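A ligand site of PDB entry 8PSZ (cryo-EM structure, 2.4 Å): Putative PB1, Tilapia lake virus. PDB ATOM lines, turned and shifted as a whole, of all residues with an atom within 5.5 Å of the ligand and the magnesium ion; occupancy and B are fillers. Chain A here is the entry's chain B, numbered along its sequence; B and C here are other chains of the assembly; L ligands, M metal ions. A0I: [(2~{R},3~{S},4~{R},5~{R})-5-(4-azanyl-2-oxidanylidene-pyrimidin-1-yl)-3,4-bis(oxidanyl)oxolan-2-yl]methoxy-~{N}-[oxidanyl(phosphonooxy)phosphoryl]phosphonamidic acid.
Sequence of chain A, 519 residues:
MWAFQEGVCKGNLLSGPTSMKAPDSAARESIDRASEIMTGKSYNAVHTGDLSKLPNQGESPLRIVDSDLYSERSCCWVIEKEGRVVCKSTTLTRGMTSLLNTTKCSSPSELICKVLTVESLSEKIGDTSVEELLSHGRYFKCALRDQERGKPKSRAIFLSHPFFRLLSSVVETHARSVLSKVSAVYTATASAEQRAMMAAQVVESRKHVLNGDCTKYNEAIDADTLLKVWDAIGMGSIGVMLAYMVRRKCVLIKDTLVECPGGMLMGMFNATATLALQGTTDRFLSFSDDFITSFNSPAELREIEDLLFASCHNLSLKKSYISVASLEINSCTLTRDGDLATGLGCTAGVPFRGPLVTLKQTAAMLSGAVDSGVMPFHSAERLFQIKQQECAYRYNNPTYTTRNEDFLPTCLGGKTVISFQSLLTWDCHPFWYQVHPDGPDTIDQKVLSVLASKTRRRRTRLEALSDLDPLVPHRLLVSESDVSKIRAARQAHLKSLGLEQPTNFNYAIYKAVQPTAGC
An oxygen (O11) of the ligand lies within salt-bridge range of the side-chain amino group (NZ) of Lys 151, at 3.3 Å. The side-chain amide nitrogen (ND2) of Asn 218 lies within hydrogen-bond range of an oxygen (O12) of the ligand (2.7 Å). OG1 of Thr 215 lies within hydrogen-bond range of O9 of the ligand (3.1 Å). A nitrogen (N3) of the ligand is in hydrogen-bond range of the side-chain carboxylate of Glu 148 (3.1 Å). O11 of the ligand lies within salt-bridge range of NH2 of Arg 155, 2.7 Å away. The backbone NH (N) of Lys 216 is in hydrogen-bond range of an oxygen (O5) of the ligand, at 3.1 Å. The backbone NH (N) of Gly 267 lies within hydrogen-bond range of an oxygen (O13) of the ligand (3.2 Å). N6 of A 21 of chain C sits at hydrogen-bond distance from a nitrogen (N3) of the ligand (3.2 Å). O6 of G 30 of chain B is in hydrogen-bond range of a nitrogen (N3) of the ligand (3.2 Å).
The side-chain hydroxyl of Tyr 217 sits at hydrogen-bond distance from the backbone carbonyl oxygen of Ser 288, at 3.4 Å. The backbone carbonyl oxygen (O) of Arg 155 lies within hydrogen-bond range of the backbone NH (N) of Arg 145 (2.9 Å). The guanidinium group (NE) of Arg 145 sits at hydrogen-bond distance from O6 of G 30 of chain B (3.2 Å). The side-chain carboxylate (OE1) of Glu 148 lies within salt-bridge range of the guanidinium group (NH2) of Arg 145 (3.8 Å). OE2 of Glu 219 sits close to OD1 of Asn 218, 3.1 Å away. NE of Arg 155 lies within salt-bridge range of OE2 of Glu 148 (2.7 Å). NH1 of Arg 155 is in hydrogen-bond range of SD of Met 266 (3.4 Å). O of Asn 218 sits at hydrogen-bond distance from N of Met 264, 2.8 Å away.
OD1 of Asp 289 lies close to O2 of the ligand, 3.2 Å away. Tyr 217 touches the ligand (N to O5, 3.7 Å). Met 266 touches the ligand. U 31 of chain B touches the ligand. Hydrophobic or aromatic side chains that line the ligand: Met 266. Along chain A the residues within 4 Å of the ligand span positions 148 to 289.
Asp 289 touches the magnesium ion (OD2 to MG, 3.2 Å). Three residues have an atom within 4 Å of the magnesium ion: Asp 213, Cys 214 and Asp 289. Along chain A the residues within 4 Å of the magnesium ion span positions 213 to 289. The nearest printed residue that does not touch the magnesium ion is Thr 215 (4.2 Å).
The magnesium ion is bound by OD2 of Asp 213 (2.1 Å), O8 of the ligand (2.1 Å) and O of Cys 214 (2.1 Å). The magnesium ion has three donor atoms within binding distance. Slightly farther from the magnesium ion lies O6 of the ligand (2.8 Å). Slightly farther from the magnesium ion lies an oxygen (O4) of the ligand (2.8 Å).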
ATOM      1  N   ARG A 145       3.097 -15.526  -2.493  1.00  0.00           N
ATOM      2  CA  ARG A 145       1.956 -15.197  -3.335  1.00  0.00           C
ATOM      3  C   ARG A 145       0.687 -15.517  -2.562  1.00  0.00           C
ATOM      4  O   ARG A 145       0.469 -16.667  -2.164  1.00  0.00           O
ATOM      5  CB  ARG A 145       2.022 -15.959  -4.663  1.00  0.00           C
ATOM      6  CG  ARG A 145       0.703 -16.108  -5.425  1.00  0.00           C
ATOM      7  CD  ARG A 145       0.527 -15.058  -6.505  1.00  0.00           C
ATOM      8  NE  ARG A 145      -0.213 -15.597  -7.646  1.00  0.00           N
ATOM      9  CZ  ARG A 145      -1.473 -15.302  -7.927  1.00  0.00           C
ATOM     10  NH1 ARG A 145      -2.192 -14.487  -7.180  1.00  0.00           N
ATOM     11  NH2 ARG A 145      -2.041 -15.856  -9.002  1.00  0.00           N
ATOM     12  N   GLU A 148      -5.088 -16.097  -3.346  1.00  0.00           N
ATOM     13  CA  GLU A 148      -5.532 -17.268  -4.082  1.00  0.00           C
ATOM     14  C   GLU A 148      -6.577 -17.996  -3.249  1.00  0.00           C
ATOM     15  O   GLU A 148      -6.282 -18.470  -2.145  1.00  0.00           O
ATOM     16  CB  GLU A 148      -4.359 -18.201  -4.397  1.00  0.00           C
ATOM     17  CG  GLU A 148      -3.289 -17.569  -5.262  1.00  0.00           C
ATOM     18  CD  GLU A 148      -2.450 -18.600  -5.990  1.00  0.00           C
ATOM     19  OE1 GLU A 148      -2.873 -19.034  -7.091  1.00  0.00           O
ATOM     20  OE2 GLU A 148      -1.391 -18.981  -5.473  1.00  0.00           O
ATOM     21  N   LYS A 151      -6.524 -21.221  -0.381  1.00  0.00           N
ATOM     22  CA  LYS A 151      -5.162 -21.420   0.119  1.00  0.00           C
ATOM     23  C   LYS A 151      -4.924 -20.461   1.278  1.00  0.00           C
ATOM     24  O   LYS A 151      -4.291 -19.409   1.100  1.00  0.00           O
ATOM     25  CB  LYS A 151      -4.124 -21.207  -0.994  1.00  0.00           C
ATOM     26  CG  LYS A 151      -4.144 -22.280  -2.069  1.00  0.00           C
ATOM     27  CD  LYS A 151      -2.797 -22.377  -2.770  1.00  0.00           C
ATOM     28  CE  LYS A 151      -1.768 -23.106  -1.918  1.00  0.00           C
ATOM     29  NZ  LYS A 151      -1.484 -24.474  -2.423  1.00  0.00           N
ATOM     30  N   ARG A 155       1.240 -19.321  -1.153  1.00  0.00           N
ATOM     31  CA  ARG A 155       2.199 -20.221  -1.778  1.00  0.00           C
ATOM     32  C   ARG A 155       3.554 -19.546  -1.940  1.00  0.00           C
ATOM     33  O   ARG A 155       3.645 -18.333  -2.168  1.00  0.00           O
ATOM     34  CB  ARG A 155       1.671 -20.727  -3.135  1.00  0.00           C
ATOM     35  CG  ARG A 155       1.908 -19.804  -4.314  1.00  0.00           C
ATOM     36  CD  ARG A 155       1.556 -20.500  -5.624  1.00  0.00           C
ATOM     37  NE  ARG A 155       0.218 -21.084  -5.585  1.00  0.00           N
ATOM     38  CZ  ARG A 155      -0.061 -22.376  -5.760  1.00  0.00           C
ATOM     39  NH1 ARG A 155       0.894 -23.272  -5.979  1.00  0.00           N
ATOM     40  NH2 ARG A 155      -1.323 -22.773  -5.717  1.00  0.00           N
ATOM     41  N   ASP A 213      -6.069 -34.944  -9.801  1.00  0.00           N
ATOM     42  CA  ASP A 213      -5.111 -33.898  -9.481  1.00  0.00           C
ATOM     43  C   ASP A 213      -3.832 -34.562  -8.975  1.00  0.00           C
ATOM     44  O   ASP A 213      -3.854 -35.697  -8.495  1.00  0.00           O
ATOM     45  CB  ASP A 213      -5.662 -32.926  -8.434  1.00  0.00           C
ATOM     46  CG  ASP A 213      -5.043 -31.538  -8.553  1.00  0.00           C
ATOM     47  OD1 ASP A 213      -5.228 -30.890  -9.596  1.00  0.00           O
ATOM     48  OD2 ASP A 213      -4.382 -31.111  -7.588  1.00  0.00           O
ATOM     49  N   CYS A 214      -2.725 -33.852  -9.105  1.00  0.00           N
ATOM     50  CA  CYS A 214      -1.431 -34.311  -8.619  1.00  0.00           C
ATOM     51  C   CYS A 214      -1.018 -33.439  -7.449  1.00  0.00           C
ATOM     52  O   CYS A 214      -1.286 -32.229  -7.434  1.00  0.00           O
ATOM     53  CB  CYS A 214      -0.373 -34.281  -9.713  1.00  0.00           C
ATOM     54  SG  CYS A 214      -0.763 -35.276 -11.171  1.00  0.00           S
ATOM     55  N   THR A 215      -0.376 -34.058  -6.465  1.00  0.00           N
ATOM     56  CA  THR A 215       0.097 -33.362  -5.282  1.00  0.00           C
ATOM     57  C   THR A 215       1.620 -33.274  -5.318  1.00  0.00           C
ATOM     58  O   THR A 215       2.291 -34.154  -5.859  1.00  0.00           O
ATOM     59  CB  THR A 215      -0.366 -34.056  -4.001  1.00  0.00           C
ATOM     60  OG1 THR A 215       0.040 -33.294  -2.852  1.00  0.00           O
ATOM     61  CG2 THR A 215       0.206 -35.472  -3.899  1.00  0.00           C
ATOM     62  N   LYS A 216       2.151 -32.201  -4.741  1.00  0.00           N
ATOM     63  CA  LYS A 216       3.600 -31.969  -4.705  1.00  0.00           C
ATOM     64  C   LYS A 216       4.184 -32.054  -6.110  1.00  0.00           C
ATOM     65  O   LYS A 216       5.232 -32.670  -6.330  1.00  0.00           O
ATOM     66  CB  LYS A 216       4.284 -32.964  -3.766  1.00  0.00           C
ATOM     67  CG  LYS A 216       3.616 -33.131  -2.413  1.00  0.00           C
ATOM     68  CD  LYS A 216       3.899 -31.961  -1.501  1.00  0.00           C
ATOM     69  CE  LYS A 216       2.702 -31.657  -0.609  1.00  0.00           C
ATOM     70  NZ  LYS A 216       2.242 -32.865   0.136  1.00  0.00           N
ATOM     71  N   TYR A 217       3.501 -31.418  -7.068  1.00  0.00           N
ATOM     72  CA  TYR A 217       3.882 -31.556  -8.467  1.00  0.00           C
ATOM     73  C   TYR A 217       5.298 -31.039  -8.705  1.00  0.00           C
ATOM     74  O   TYR A 217       6.132 -31.745  -9.293  1.00  0.00           O
ATOM     75  CB  TYR A 217       2.889 -30.800  -9.340  1.00  0.00           C
ATOM     76  CG  TYR A 217       3.009 -31.124 -10.813  1.00  0.00           C
ATOM     77  CD1 TYR A 217       2.760 -32.411 -11.279  1.00  0.00           C
ATOM     78  CD2 TYR A 217       3.372 -30.148 -11.726  1.00  0.00           C
ATOM     79  CE1 TYR A 217       2.861 -32.704 -12.622  1.00  0.00           C
ATOM     80  CE2 TYR A 217       3.472 -30.440 -13.069  1.00  0.00           C
ATOM     81  CZ  TYR A 217       3.220 -31.717 -13.506  1.00  0.00           C
ATOM     82  OH  TYR A 217       3.327 -32.016 -14.846  1.00  0.00           O
ATOM     83  N   ASN A 218       5.598 -29.819  -8.265  1.00  0.00           N
ATOM     84  CA  ASN A 218       6.896 -29.242  -8.565  1.00  0.00           C
ATOM     85  C   ASN A 218       7.990 -29.854  -7.704  1.00  0.00           C
ATOM     86  O   ASN A 218       9.158 -29.866  -8.117  1.00  0.00           O
ATOM     87  CB  ASN A 218       6.846 -27.719  -8.380  1.00  0.00           C
ATOM     88  CG  ASN A 218       6.735 -27.305  -6.926  1.00  0.00           C
ATOM     89  OD1 ASN A 218       7.749 -27.171  -6.234  1.00  0.00           O
ATOM     90  ND2 ASN A 218       5.512 -27.095  -6.462  1.00  0.00           N
ATOM     91  N   GLU A 219       7.648 -30.366  -6.520  1.00  0.00           N
ATOM     92  CA  GLU A 219       8.625 -31.010  -5.667  1.00  0.00           C
ATOM     93  C   GLU A 219       8.996 -32.407  -6.136  1.00  0.00           C
ATOM     94  O   GLU A 219      10.056 -32.912  -5.742  1.00  0.00           O
ATOM     95  CB  GLU A 219       8.108 -31.083  -4.227  1.00  0.00           C
ATOM     96  CG  GLU A 219       8.163 -29.780  -3.460  1.00  0.00           C
ATOM     97  CD  GLU A 219       6.940 -28.899  -3.682  1.00  0.00           C
ATOM     98  OE1 GLU A 219       5.946 -29.395  -4.257  1.00  0.00           O
ATOM     99  OE2 GLU A 219       6.971 -27.717  -3.284  1.00  0.00           O
ATOM    100  N   MET A 264      11.554 -28.718  -8.888  1.00  0.00           N
ATOM    101  CA  MET A 264      11.817 -27.691  -9.888  1.00  0.00           C
ATOM    102  C   MET A 264      11.343 -26.302  -9.467  1.00  0.00           C
ATOM    103  O   MET A 264      11.290 -25.395 -10.300  1.00  0.00           O
ATOM    104  CB  MET A 264      11.179 -28.063 -11.238  1.00  0.00           C
ATOM    105  CG  MET A 264       9.694 -28.348 -11.184  1.00  0.00           C
ATOM    106  SD  MET A 264       8.985 -28.505 -12.835  1.00  0.00           S
ATOM    107  CE  MET A 264       7.260 -28.166 -12.509  1.00  0.00           C
ATOM    108  N   MET A 266       8.339 -24.755  -8.041  1.00  0.00           N
ATOM    109  CA  MET A 266       7.040 -24.112  -8.219  1.00  0.00           C
ATOM    110  C   MET A 266       6.807 -23.690  -9.670  1.00  0.00           C
ATOM    111  O   MET A 266       6.773 -22.504 -10.026  1.00  0.00           O
ATOM    112  CB  MET A 266       6.902 -22.917  -7.272  1.00  0.00           C
ATOM    113  CG  MET A 266       5.521 -22.269  -7.245  1.00  0.00           C
ATOM    114  SD  MET A 266       4.195 -23.374  -6.727  1.00  0.00           S
ATOM    115  CE  MET A 266       4.792 -23.912  -5.136  1.00  0.00           C
ATOM    116  N   GLY A 267       6.667 -24.700 -10.528  1.00  0.00           N
ATOM    117  CA  GLY A 267       6.227 -24.478 -11.891  1.00  0.00           C
ATOM    118  C   GLY A 267       7.219 -23.772 -12.783  1.00  0.00           C
ATOM    119  O   GLY A 267       6.827 -22.900 -13.566  1.00  0.00           O
ATOM    120  N   ASN A 270       6.487 -26.075 -16.855  1.00  0.00           N
ATOM    121  CA  ASN A 270       5.160 -26.669 -16.951  1.00  0.00           C
ATOM    122  C   ASN A 270       5.049 -27.596 -18.153  1.00  0.00           C
ATOM    123  O   ASN A 270       4.541 -28.718 -18.038  1.00  0.00           O
ATOM    124  CB  ASN A 270       4.088 -25.573 -17.027  1.00  0.00           C
ATOM    125  CG  ASN A 270       4.031 -24.740 -15.757  1.00  0.00           C
ATOM    126  OD1 ASN A 270       3.983 -25.263 -14.656  1.00  0.00           O
ATOM    127  ND2 ASN A 270       4.045 -23.420 -15.920  1.00  0.00           N
ATOM    128  N   SER A 288       0.156 -29.917 -16.990  1.00  0.00           N
ATOM    129  CA  SER A 288       0.688 -29.734 -15.645  1.00  0.00           C
ATOM    130  C   SER A 288       0.006 -30.752 -14.737  1.00  0.00           C
ATOM    131  O   SER A 288      -0.089 -31.934 -15.127  1.00  0.00           O
ATOM    132  CB  SER A 288       0.507 -28.272 -15.253  1.00  0.00           C
ATOM    133  OG  SER A 288       1.148 -27.987 -14.020  1.00  0.00           O
ATOM    134  N   ASP A 289      -0.465 -30.374 -13.553  1.00  0.00           N
ATOM    135  CA  ASP A 289      -1.056 -31.320 -12.599  1.00  0.00           C
ATOM    136  C   ASP A 289      -2.579 -31.318 -12.682  1.00  0.00           C
ATOM    137  O   ASP A 289      -3.265 -31.062 -11.691  1.00  0.00           O
ATOM    138  CB  ASP A 289      -0.595 -30.980 -11.193  1.00  0.00           C
ATOM    139  CG  ASP A 289      -0.882 -29.543 -10.816  1.00  0.00           C
ATOM    140  OD1 ASP A 289      -0.066 -28.669 -11.172  1.00  0.00           O
ATOM    141  OD2 ASP A 289      -1.927 -29.293 -10.184  1.00  0.00           O
ATOM    142  N   SER A 316      -3.086 -37.223  -6.318  1.00  0.00           N
ATOM    143  CA  SER A 316      -3.516 -36.613  -5.062  1.00  0.00           C
ATOM    144  C   SER A 316      -4.709 -37.393  -4.536  1.00  0.00           C
ATOM    145  O   SER A 316      -5.808 -37.304  -5.095  1.00  0.00           O
ATOM    146  CB  SER A 316      -3.864 -35.142  -5.271  1.00  0.00           C
ATOM    147  OG  SER A 316      -4.570 -34.627  -4.148  1.00  0.00           O
ATOM    148  N   LYS A 318      -6.190 -36.859  -1.781  1.00  0.00           N
ATOM    149  CA  LYS A 318      -7.093 -35.973  -1.058  1.00  0.00           C
ATOM    150  C   LYS A 318      -8.185 -35.432  -1.973  1.00  0.00           C
ATOM    151  O   LYS A 318      -9.354 -35.350  -1.569  1.00  0.00           O
ATOM    152  CB  LYS A 318      -6.303 -34.825  -0.438  1.00  0.00           C
ATOM    153  CG  LYS A 318      -7.031 -34.104   0.683  1.00  0.00           C
ATOM    154  CD  LYS A 318      -6.738 -32.614   0.678  1.00  0.00           C
ATOM    155  CE  LYS A 318      -5.380 -32.307   1.283  1.00  0.00           C
ATOM    156  NZ  LYS A 318      -4.703 -31.181   0.596  1.00  0.00           N
ATOM    157  N   LYS A 319      -7.839 -35.062  -3.202  1.00  0.00           N
ATOM    158  CA  LYS A 319      -8.742 -34.318  -4.073  1.00  0.00           C
ATOM    159  C   LYS A 319      -9.216 -35.085  -5.301  1.00  0.00           C
ATOM    160  O   LYS A 319     -10.274 -34.770  -5.831  1.00  0.00           O
ATOM    161  CB  LYS A 319      -8.067 -33.019  -4.535  1.00  0.00           C
ATOM    162  CG  LYS A 319      -7.550 -32.164  -3.399  1.00  0.00           C
ATOM    163  CD  LYS A 319      -7.210 -30.762  -3.849  1.00  0.00           C
ATOM    164  CE  LYS A 319      -6.848 -29.876  -2.666  1.00  0.00           C
ATOM    165  NZ  LYS A 319      -6.703 -28.449  -3.062  1.00  0.00           N
ATOM    166  P     G B  30       6.105 -11.010  -9.943  1.00  0.00           P
ATOM    167  OP1   G B  30       6.808  -9.709  -9.922  1.00  0.00           O
ATOM    168  OP2   G B  30       4.698 -11.082 -10.435  1.00  0.00           O
ATOM    169  O5'   G B  30       6.963 -12.030 -10.805  1.00  0.00           O
ATOM    170  C5'   G B  30       8.308 -12.320 -10.450  1.00  0.00           C
ATOM    171  C4'   G B  30       8.596 -13.793 -10.511  1.00  0.00           C
ATOM    172  O4'   G B  30       8.008 -14.471  -9.365  1.00  0.00           O
ATOM    173  C3'   G B  30       8.035 -14.557 -11.707  1.00  0.00           C
ATOM    174  O3'   G B  30       8.818 -14.392 -12.877  1.00  0.00           O
ATOM    175  C2'   G B  30       7.975 -15.987 -11.193  1.00  0.00           C
ATOM    176  O2'   G B  30       9.246 -16.599 -11.255  1.00  0.00           O
ATOM    177  C1'   G B  30       7.595 -15.769  -9.729  1.00  0.00           C
ATOM    178  N9    G B  30       6.148 -15.895  -9.499  1.00  0.00           N
ATOM    179  C8    G B  30       5.280 -14.908  -9.098  1.00  0.00           C
ATOM    180  N7    G B  30       4.050 -15.322  -8.976  1.00  0.00           N
ATOM    181  C5    G B  30       4.108 -16.659  -9.322  1.00  0.00           C
ATOM    182  C6    G B  30       3.089 -17.650  -9.381  1.00  0.00           C
ATOM    183  O6    G B  30       1.896 -17.518  -9.132  1.00  0.00           O
ATOM    184  N1    G B  30       3.592 -18.880  -9.790  1.00  0.00           N
ATOM    185  C2    G B  30       4.894 -19.138 -10.089  1.00  0.00           C
ATOM    186  N2    G B  30       5.191 -20.396 -10.464  1.00  0.00           N
ATOM    187  N3    G B  30       5.862 -18.235 -10.038  1.00  0.00           N
ATOM    188  C4    G B  30       5.389 -17.028  -9.647  1.00  0.00           C
ATOM    189  P     U B  31       8.124 -14.442 -14.321  1.00  0.00           P
ATOM    190  OP1   U B  31       9.141 -14.058 -15.324  1.00  0.00           O
ATOM    191  OP2   U B  31       6.847 -13.679 -14.248  1.00  0.00           O
ATOM    192  O5'   U B  31       7.744 -15.976 -14.525  1.00  0.00           O
ATOM    193  C5'   U B  31       8.749 -16.980 -14.550  1.00  0.00           C
ATOM    194  C4'   U B  31       8.143 -18.336 -14.786  1.00  0.00           C
ATOM    195  O4'   U B  31       7.419 -18.769 -13.603  1.00  0.00           O
ATOM    196  C3'   U B  31       7.119 -18.420 -15.897  1.00  0.00           C
ATOM    197  O3'   U B  31       7.692 -18.490 -17.190  1.00  0.00           O
ATOM    198  C2'   U B  31       6.317 -19.646 -15.512  1.00  0.00           C
ATOM    199  O2'   U B  31       6.989 -20.845 -15.873  1.00  0.00           O
ATOM    200  C1'   U B  31       6.291 -19.521 -13.991  1.00  0.00           C
ATOM    201  N1    U B  31       5.065 -18.844 -13.501  1.00  0.00           N
ATOM    202  C2    U B  31       3.916 -19.599 -13.435  1.00  0.00           C
ATOM    203  O2    U B  31       3.867 -20.765 -13.767  1.00  0.00           O
ATOM    204  N3    U B  31       2.814 -18.916 -12.975  1.00  0.00           N
ATOM    205  C4    U B  31       2.756 -17.602 -12.584  1.00  0.00           C
ATOM    206  O4    U B  31       1.685 -17.134 -12.193  1.00  0.00           O
ATOM    207  C5    U B  31       3.992 -16.891 -12.677  1.00  0.00           C
ATOM    208  C6    U B  31       5.080 -17.523 -13.126  1.00  0.00           C
ATOM    209  P     A C  21      -7.808 -24.103 -10.924  1.00  0.00           P
ATOM    210  OP1   A C  21      -8.541 -25.327 -10.525  1.00  0.00           O
ATOM    211  OP2   A C  21      -7.708 -22.968  -9.978  1.00  0.00           O
ATOM    212  O5'   A C  21      -6.334 -24.525 -11.354  1.00  0.00           O
ATOM    213  C5'   A C  21      -6.119 -25.542 -12.315  1.00  0.00           C
ATOM    214  C4'   A C  21      -4.648 -25.733 -12.615  1.00  0.00           C
ATOM    215  O4'   A C  21      -4.150 -24.597 -13.369  1.00  0.00           O
ATOM    216  C3'   A C  21      -3.723 -25.796 -11.414  1.00  0.00           C
ATOM    217  O3'   A C  21      -3.720 -27.075 -10.788  1.00  0.00           O
ATOM    218  C2'   A C  21      -2.381 -25.415 -12.006  1.00  0.00           C
ATOM    219  O2'   A C  21      -1.768 -26.518 -12.658  1.00  0.00           O
ATOM    220  C1'   A C  21      -2.791 -24.380 -13.063  1.00  0.00           C
ATOM    221  N9    A C  21      -2.611 -22.993 -12.593  1.00  0.00           N
ATOM    222  C8    A C  21      -3.505 -22.163 -11.967  1.00  0.00           C
ATOM    223  N7    A C  21      -3.019 -20.980 -11.679  1.00  0.00           N
ATOM    224  C5    A C  21      -1.716 -21.032 -12.144  1.00  0.00           C
ATOM    225  C6    A C  21      -0.669 -20.093 -12.154  1.00  0.00           C
ATOM    226  N6    A C  21      -0.763 -18.863 -11.647  1.00  0.00           N
ATOM    227  N1    A C  21       0.505 -20.472 -12.701  1.00  0.00           N
ATOM    228  C2    A C  21       0.606 -21.708 -13.204  1.00  0.00           C
ATOM    229  N3    A C  21      -0.303 -22.674 -13.258  1.00  0.00           N
ATOM    230  C4    A C  21      -1.451 -22.265 -12.706  1.00  0.00           C
HETATM  231  C1  A0I L   1      -0.659 -22.209  -9.002  1.00  0.00           C
HETATM  232  C2  A0I L   1      -0.144 -23.378  -9.435  1.00  0.00           C
HETATM  233  C3  A0I L   1       1.934 -22.310  -9.959  1.00  0.00           C
HETATM  234  C4  A0I L   1       0.175 -21.064  -9.042  1.00  0.00           C
HETATM  235  C5  A0I L   1       1.685 -24.742 -10.397  1.00  0.00           C
HETATM  236  C6  A0I L   1       2.957 -25.204  -9.662  1.00  0.00           C
HETATM  237  C7  A0I L   1       2.342 -26.043  -8.537  1.00  0.00           C
HETATM  238  C8  A0I L   1       1.218 -26.751  -9.295  1.00  0.00           C
HETATM  239  C9  A0I L   1       0.131 -27.341  -8.431  1.00  0.00           C
HETATM  240  N1  A0I L   1       1.127 -23.453  -9.909  1.00  0.00           N
HETATM  241  N2  A0I L   1       1.428 -21.139  -9.512  1.00  0.00           N
HETATM  242  N3  A0I L   1      -0.268 -19.889  -8.625  1.00  0.00           N
HETATM  243  N4  A0I L   1      -0.100 -27.515  -5.229  1.00  0.00           N
HETATM  244  O1  A0I L   1       3.084 -22.410 -10.389  1.00  0.00           O
HETATM  245  O10 A0I L   1      -2.394 -28.689  -3.074  1.00  0.00           O
HETATM  246  O11 A0I L   1      -1.587 -25.442  -5.572  1.00  0.00           O
HETATM  247  O12 A0I L   1       3.245 -26.959  -7.945  1.00  0.00           O
HETATM  248  O13 A0I L   1       3.743 -25.985 -10.538  1.00  0.00           O
HETATM  249  O2  A0I L   1       0.713 -25.733 -10.192  1.00  0.00           O
HETATM  250  O3  A0I L   1      -0.357 -26.348  -7.503  1.00  0.00           O
HETATM  251  O4  A0I L   1      -2.279 -27.665  -6.675  1.00  0.00           O
HETATM  252  O5  A0I L   1       1.844 -29.116  -4.679  1.00  0.00           O
HETATM  253  O6  A0I L   1       0.171 -29.789  -6.526  1.00  0.00           O
HETATM  254  O7  A0I L   1      -0.411 -29.816  -4.149  1.00  0.00           O
HETATM  255  O8  A0I L   1      -2.670 -30.011  -5.222  1.00  0.00           O
HETATM  256  O9  A0I L   1      -2.179 -31.187  -3.052  1.00  0.00           O
HETATM  257  P1  A0I L   1      -1.196 -26.745  -6.196  1.00  0.00           P
HETATM  258  P2  A0I L   1       0.458 -29.056  -5.255  1.00  0.00           P
HETATM  259  P3  A0I L   1      -2.003 -29.922  -3.857  1.00  0.00           P
HETATM  260 MG    MG M   1      -2.452 -30.448  -7.234  1.00  0.00          MG
